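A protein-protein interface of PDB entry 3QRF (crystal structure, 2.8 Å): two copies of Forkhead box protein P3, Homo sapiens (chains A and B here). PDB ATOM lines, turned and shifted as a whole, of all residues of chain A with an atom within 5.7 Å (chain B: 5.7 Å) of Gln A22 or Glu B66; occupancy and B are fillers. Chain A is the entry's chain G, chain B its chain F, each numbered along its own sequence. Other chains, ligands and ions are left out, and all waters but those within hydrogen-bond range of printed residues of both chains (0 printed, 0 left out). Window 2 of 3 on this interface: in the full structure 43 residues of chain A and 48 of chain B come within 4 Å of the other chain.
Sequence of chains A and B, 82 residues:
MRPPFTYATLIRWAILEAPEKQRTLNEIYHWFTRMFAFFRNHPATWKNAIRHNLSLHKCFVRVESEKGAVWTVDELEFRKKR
Of the printed residues of chain B, Ile A15 touches Trp B71 (3.6 Å) and Thr B72 (3.97 Å).
Gln A22 touches just these residues of chain B: Ser B65 (3.2 Å), Glu B66 (3.0 Å), Val B70 (3.6 Å), Trp B71 (3.1 Å) and Thr B72 (3.5 Å).
Printed residues of chain A within 4 Å of Ser B65: Gln A22.
Of chain A, only Gln A22 (3.0 Å) comes within 4 Å of Glu B66.
Printed residues of chain A within 4 Å of Lys B67: Glu A27 (3.3 Å).
Printed residues of chain A within 4 Å of Val B70: Gln A22 and Arg A23.
No position is printed for both chains.
Printed residues of chain A that touch a printed residue of chain B: Ile A15, Gln A22, Arg A23 and Glu A27.
Hydrophobic or aromatic side chains of chain A that line the printed part of chain B: Ile A15.
Of the 10 printed residues of chain B, 6 touch a printed residue of chain A.
Printed residues of chain B that touch a printed residue of chain A: Ser B65, Glu B66, Lys B67, Val B70, Trp B71 and Thr B72.
The side-chain hydroxyl (OG) of Ser B65 sits close to the side-chain carboxylate (OE2) of Glu B66 (3.1 Å).
The backbone NH of Val B63 lies within hydrogen-bond range of the backbone carbonyl oxygen of Val B70 (2.9 Å).
OE2 of Glu A27 sits at hydrogen-bond distance from N of Thr A24.
The side-chain amino group (NZ) of Lys B67 is in salt-bridge range of the side-chain carboxylate (OE1) of Glu A27 (3.3 Å).
The backbone NH (N) of Arg A23 lies within hydrogen-bond range of the backbone carbonyl oxygen (O) of Trp B71 (2.9 Å).
OE1 of Gln A22 sits at hydrogen-bond distance from OG of Ser B65.
OE1 of Gln A22 sits close to OE2 of Glu B66 (3.0 Å).
Among the printed residues, pairs that only touch across the chains: Gln A22 with Trp B71 (3.1 Å), Arg A23 with Val B70 (3.2 Å), Gln A22 with Thr B72 (3.5 Å), Gln A22 with Val B70 (3.6 Å), Ile A15 with Trp B71 (3.6 Å) and Ile A15 with Thr B72 (3.97 Å).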
ATOM      1  N   ILE A  15     -23.922   7.035   4.084  1.00  0.00           N
ATOM      2  CA  ILE A  15     -24.503   6.815   2.776  1.00  0.00           C
ATOM      3  C   ILE A  15     -25.507   7.917   2.486  1.00  0.00           C
ATOM      4  O   ILE A  15     -25.734   8.252   1.329  1.00  0.00           O
ATOM      5  CB  ILE A  15     -25.206   5.448   2.666  1.00  0.00           C
ATOM      6  CG1 ILE A  15     -24.214   4.317   2.895  1.00  0.00           C
ATOM      7  CG2 ILE A  15     -25.779   5.271   1.285  1.00  0.00           C
ATOM      8  CD1 ILE A  15     -24.852   2.972   2.755  1.00  0.00           C
ATOM      9  N   ALA A  18     -24.654  11.732   1.418  1.00  0.00           N
ATOM     10  CA  ALA A  18     -24.409  11.829  -0.011  1.00  0.00           C
ATOM     11  C   ALA A  18     -25.748  11.996  -0.706  1.00  0.00           C
ATOM     12  O   ALA A  18     -26.604  11.117  -0.647  1.00  0.00           O
ATOM     13  CB  ALA A  18     -23.713  10.580  -0.500  1.00  0.00           C
ATOM     14  N   PRO A  19     -25.935  13.126  -1.397  1.00  0.00           N
ATOM     15  CA  PRO A  19     -27.190  13.419  -2.106  1.00  0.00           C
ATOM     16  C   PRO A  19     -27.767  12.244  -2.894  1.00  0.00           C
ATOM     17  O   PRO A  19     -28.991  12.058  -2.948  1.00  0.00           O
ATOM     18  CB  PRO A  19     -26.813  14.591  -3.009  1.00  0.00           C
ATOM     19  CG  PRO A  19     -25.670  15.270  -2.257  1.00  0.00           C
ATOM     20  CD  PRO A  19     -24.874  14.086  -1.762  1.00  0.00           C
ATOM     21  N   GLU A  20     -26.882  11.452  -3.492  1.00  0.00           N
ATOM     22  CA  GLU A  20     -27.285  10.302  -4.290  1.00  0.00           C
ATOM     23  C   GLU A  20     -27.977   9.197  -3.470  1.00  0.00           C
ATOM     24  O   GLU A  20     -28.656   8.323  -4.030  1.00  0.00           O
ATOM     25  CB  GLU A  20     -26.056   9.736  -5.010  1.00  0.00           C
ATOM     26  CG  GLU A  20     -25.338  10.748  -5.896  1.00  0.00           C
ATOM     27  CD  GLU A  20     -24.301  11.609  -5.155  1.00  0.00           C
ATOM     28  OE1 GLU A  20     -24.582  12.082  -4.026  1.00  0.00           O
ATOM     29  OE2 GLU A  20     -23.201  11.827  -5.725  1.00  0.00           O
ATOM     30  N   LYS A  21     -27.820   9.261  -2.146  1.00  0.00           N
ATOM     31  CA  LYS A  21     -28.395   8.275  -1.225  1.00  0.00           C
ATOM     32  C   LYS A  21     -27.780   6.912  -1.485  1.00  0.00           C
ATOM     33  O   LYS A  21     -28.388   5.868  -1.201  1.00  0.00           O
ATOM     34  CB  LYS A  21     -29.917   8.182  -1.367  1.00  0.00           C
ATOM     35  CG  LYS A  21     -30.680   9.338  -0.732  1.00  0.00           C
ATOM     36  CD  LYS A  21     -32.153   8.986  -0.560  1.00  0.00           C
ATOM     37  CE  LYS A  21     -32.962  10.184  -0.080  1.00  0.00           C
ATOM     38  NZ  LYS A  21     -32.941  11.299  -1.080  1.00  0.00           N
ATOM     39  N   GLN A  22     -26.561   6.953  -2.023  1.00  0.00           N
ATOM     40  CA  GLN A  22     -25.782   5.771  -2.348  1.00  0.00           C
ATOM     41  C   GLN A  22     -24.304   6.160  -2.496  1.00  0.00           C
ATOM     42  O   GLN A  22     -23.970   7.158  -3.143  1.00  0.00           O
ATOM     43  CB  GLN A  22     -26.301   5.149  -3.643  1.00  0.00           C
ATOM     44  CG  GLN A  22     -26.083   6.002  -4.879  1.00  0.00           C
ATOM     45  CD  GLN A  22     -26.548   5.318  -6.154  1.00  0.00           C
ATOM     46  OE1 GLN A  22     -25.924   5.470  -7.201  1.00  0.00           O
ATOM     47  NE2 GLN A  22     -27.653   4.569  -6.077  1.00  0.00           N
ATOM     48  N   ARG A  23     -23.422   5.369  -1.894  1.00  0.00           N
ATOM     49  CA  ARG A  23     -21.985   5.638  -1.950  1.00  0.00           C
ATOM     50  C   ARG A  23     -21.143   4.377  -2.163  1.00  0.00           C
ATOM     51  O   ARG A  23     -21.634   3.256  -2.024  1.00  0.00           O
ATOM     52  CB  ARG A  23     -21.519   6.316  -0.657  1.00  0.00           C
ATOM     53  CG  ARG A  23     -22.072   7.704  -0.421  1.00  0.00           C
ATOM     54  CD  ARG A  23     -20.943   8.702  -0.261  1.00  0.00           C
ATOM     55  NE  ARG A  23     -21.077   9.473   0.964  1.00  0.00           N
ATOM     56  CZ  ARG A  23     -20.107  10.226   1.469  1.00  0.00           C
ATOM     57  NH1 ARG A  23     -18.937  10.304   0.846  1.00  0.00           N
ATOM     58  NH2 ARG A  23     -20.300  10.892   2.601  1.00  0.00           N
ATOM     59  N   THR A  24     -19.870   4.578  -2.492  1.00  0.00           N
ATOM     60  CA  THR A  24     -18.946   3.475  -2.705  1.00  0.00           C
ATOM     61  C   THR A  24     -18.217   3.228  -1.401  1.00  0.00           C
ATOM     62  O   THR A  24     -18.170   4.099  -0.540  1.00  0.00           O
ATOM     63  CB  THR A  24     -17.883   3.806  -3.733  1.00  0.00           C
ATOM     64  OG1 THR A  24     -16.833   4.551  -3.097  1.00  0.00           O
ATOM     65  CG2 THR A  24     -18.479   4.615  -4.864  1.00  0.00           C
ATOM     66  N   GLU A  27     -15.727   5.930  -0.500  1.00  0.00           N
ATOM     67  CA  GLU A  27     -16.384   7.152  -0.071  1.00  0.00           C
ATOM     68  C   GLU A  27     -16.805   6.990   1.395  1.00  0.00           C
ATOM     69  O   GLU A  27     -16.522   7.853   2.225  1.00  0.00           O
ATOM     70  CB  GLU A  27     -17.583   7.437  -0.985  1.00  0.00           C
ATOM     71  CG  GLU A  27     -17.157   8.020  -2.338  1.00  0.00           C
ATOM     72  CD  GLU A  27     -18.157   7.764  -3.467  1.00  0.00           C
ATOM     73  OE1 GLU A  27     -17.904   8.243  -4.601  1.00  0.00           O
ATOM     74  OE2 GLU A  27     -19.187   7.086  -3.231  1.00  0.00           O
ATOM     75  N   VAL B  63     -25.562  -2.133  -5.097  1.00  0.00           N
ATOM     76  CA  VAL B  63     -26.228  -2.089  -6.390  1.00  0.00           C
ATOM     77  C   VAL B  63     -25.188  -1.758  -7.447  1.00  0.00           C
ATOM     78  O   VAL B  63     -24.190  -1.088  -7.156  1.00  0.00           O
ATOM     79  CB  VAL B  63     -27.355  -1.028  -6.408  1.00  0.00           C
ATOM     80  CG1 VAL B  63     -28.235  -1.179  -5.176  1.00  0.00           C
ATOM     81  CG2 VAL B  63     -26.766   0.370  -6.470  1.00  0.00           C
ATOM     82  N   GLU B  64     -25.427  -2.230  -8.669  1.00  0.00           N
ATOM     83  CA  GLU B  64     -24.503  -2.026  -9.785  1.00  0.00           C
ATOM     84  C   GLU B  64     -24.736  -0.700 -10.483  1.00  0.00           C
ATOM     85  O   GLU B  64     -24.127  -0.413 -11.516  1.00  0.00           O
ATOM     86  CB  GLU B  64     -24.623  -3.182 -10.803  1.00  0.00           C
ATOM     87  CG  GLU B  64     -26.002  -3.350 -11.486  1.00  0.00           C
ATOM     88  CD  GLU B  64     -27.131  -3.855 -10.556  1.00  0.00           C
ATOM     89  OE1 GLU B  64     -28.286  -3.977 -11.033  1.00  0.00           O
ATOM     90  OE2 GLU B  64     -26.880  -4.138  -9.360  1.00  0.00           O
ATOM     91  N   SER B  65     -25.599   0.117  -9.896  1.00  0.00           N
ATOM     92  CA  SER B  65     -25.937   1.411 -10.478  1.00  0.00           C
ATOM     93  C   SER B  65     -24.759   2.323 -10.830  1.00  0.00           C
ATOM     94  O   SER B  65     -23.608   2.062 -10.473  1.00  0.00           O
ATOM     95  CB  SER B  65     -26.920   2.163  -9.562  1.00  0.00           C
ATOM     96  OG  SER B  65     -26.320   2.528  -8.328  1.00  0.00           O
ATOM     97  N   GLU B  66     -25.088   3.386 -11.563  1.00  0.00           N
ATOM     98  CA  GLU B  66     -24.151   4.414 -12.018  1.00  0.00           C
ATOM     99  C   GLU B  66     -22.717   3.965 -12.327  1.00  0.00           C
ATOM    100  O   GLU B  66     -22.480   2.842 -12.772  1.00  0.00           O
ATOM    101  CB  GLU B  66     -24.127   5.578 -11.002  1.00  0.00           C
ATOM    102  CG  GLU B  66     -25.263   6.616 -11.170  1.00  0.00           C
ATOM    103  CD  GLU B  66     -26.635   6.122 -10.707  1.00  0.00           C
ATOM    104  OE1 GLU B  66     -27.640   6.831 -10.957  1.00  0.00           O
ATOM    105  OE2 GLU B  66     -26.714   5.038 -10.083  1.00  0.00           O
ATOM    106  N   LYS B  67     -21.782   4.885 -12.107  1.00  0.00           N
ATOM    107  CA  LYS B  67     -20.353   4.681 -12.319  1.00  0.00           C
ATOM    108  C   LYS B  67     -19.844   3.281 -11.971  1.00  0.00           C
ATOM    109  O   LYS B  67     -19.358   2.556 -12.851  1.00  0.00           O
ATOM    110  CB  LYS B  67     -19.586   5.727 -11.509  1.00  0.00           C
ATOM    111  CG  LYS B  67     -20.233   6.047 -10.157  1.00  0.00           C
ATOM    112  CD  LYS B  67     -19.569   7.243  -9.478  1.00  0.00           C
ATOM    113  CE  LYS B  67     -20.275   7.622  -8.180  1.00  0.00           C
ATOM    114  NZ  LYS B  67     -19.558   8.708  -7.449  1.00  0.00           N
ATOM    115  N   GLY B  68     -19.944   2.911 -10.692  1.00  0.00           N
ATOM    116  CA  GLY B  68     -19.502   1.598 -10.251  1.00  0.00           C
ATOM    117  C   GLY B  68     -20.416   1.047  -9.171  1.00  0.00           C
ATOM    118  O   GLY B  68     -21.450   1.640  -8.876  1.00  0.00           O
ATOM    119  N   ALA B  69     -20.048  -0.088  -8.581  1.00  0.00           N
ATOM    120  CA  ALA B  69     -20.859  -0.691  -7.525  1.00  0.00           C
ATOM    121  C   ALA B  69     -20.881   0.274  -6.361  1.00  0.00           C
ATOM    122  O   ALA B  69     -19.841   0.778  -5.937  1.00  0.00           O
ATOM    123  CB  ALA B  69     -20.265  -2.028  -7.085  1.00  0.00           C
ATOM    124  N   VAL B  70     -22.072   0.534  -5.846  1.00  0.00           N
ATOM    125  CA  VAL B  70     -22.214   1.463  -4.741  1.00  0.00           C
ATOM    126  C   VAL B  70     -23.093   0.876  -3.657  1.00  0.00           C
ATOM    127  O   VAL B  70     -23.900  -0.025  -3.912  1.00  0.00           O
ATOM    128  CB  VAL B  70     -22.849   2.800  -5.205  1.00  0.00           C
ATOM    129  CG1 VAL B  70     -22.031   3.396  -6.325  1.00  0.00           C
ATOM    130  CG2 VAL B  70     -24.287   2.574  -5.663  1.00  0.00           C
ATOM    131  N   TRP B  71     -22.946   1.396  -2.449  1.00  0.00           N
ATOM    132  CA  TRP B  71     -23.740   0.921  -1.334  1.00  0.00           C
ATOM    133  C   TRP B  71     -24.981   1.781  -1.101  1.00  0.00           C
ATOM    134  O   TRP B  71     -24.980   2.973  -1.387  1.00  0.00           O
ATOM    135  CB  TRP B  71     -22.876   0.867  -0.079  1.00  0.00           C
ATOM    136  CG  TRP B  71     -21.985  -0.310  -0.062  1.00  0.00           C
ATOM    137  CD1 TRP B  71     -20.660  -0.341  -0.355  1.00  0.00           C
ATOM    138  CD2 TRP B  71     -22.359  -1.647   0.279  1.00  0.00           C
ATOM    139  NE1 TRP B  71     -20.176  -1.625  -0.212  1.00  0.00           N
ATOM    140  CE2 TRP B  71     -21.204  -2.444   0.178  1.00  0.00           C
ATOM    141  CE3 TRP B  71     -23.564  -2.251   0.665  1.00  0.00           C
ATOM    142  CZ2 TRP B  71     -21.215  -3.813   0.454  1.00  0.00           C
ATOM    143  CZ3 TRP B  71     -23.570  -3.617   0.939  1.00  0.00           C
ATOM    144  CH2 TRP B  71     -22.406  -4.379   0.834  1.00  0.00           C
ATOM    145  N   THR B  72     -26.040   1.176  -0.583  1.00  0.00           N
ATOM    146  CA  THR B  72     -27.279   1.912  -0.343  1.00  0.00           C
ATOM    147  C   THR B  72     -28.059   1.365   0.847  1.00  0.00           C
ATOM    148  O   THR B  72     -27.899   0.207   1.241  1.00  0.00           O
ATOM    149  CB  THR B  72     -28.229   1.810  -1.531  1.00  0.00           C
ATOM    150  OG1 THR B  72     -28.912   0.549  -1.458  1.00  0.00           O
ATOM    151  CG2 THR B  72     -27.462   1.912  -2.848  1.00  0.00           C
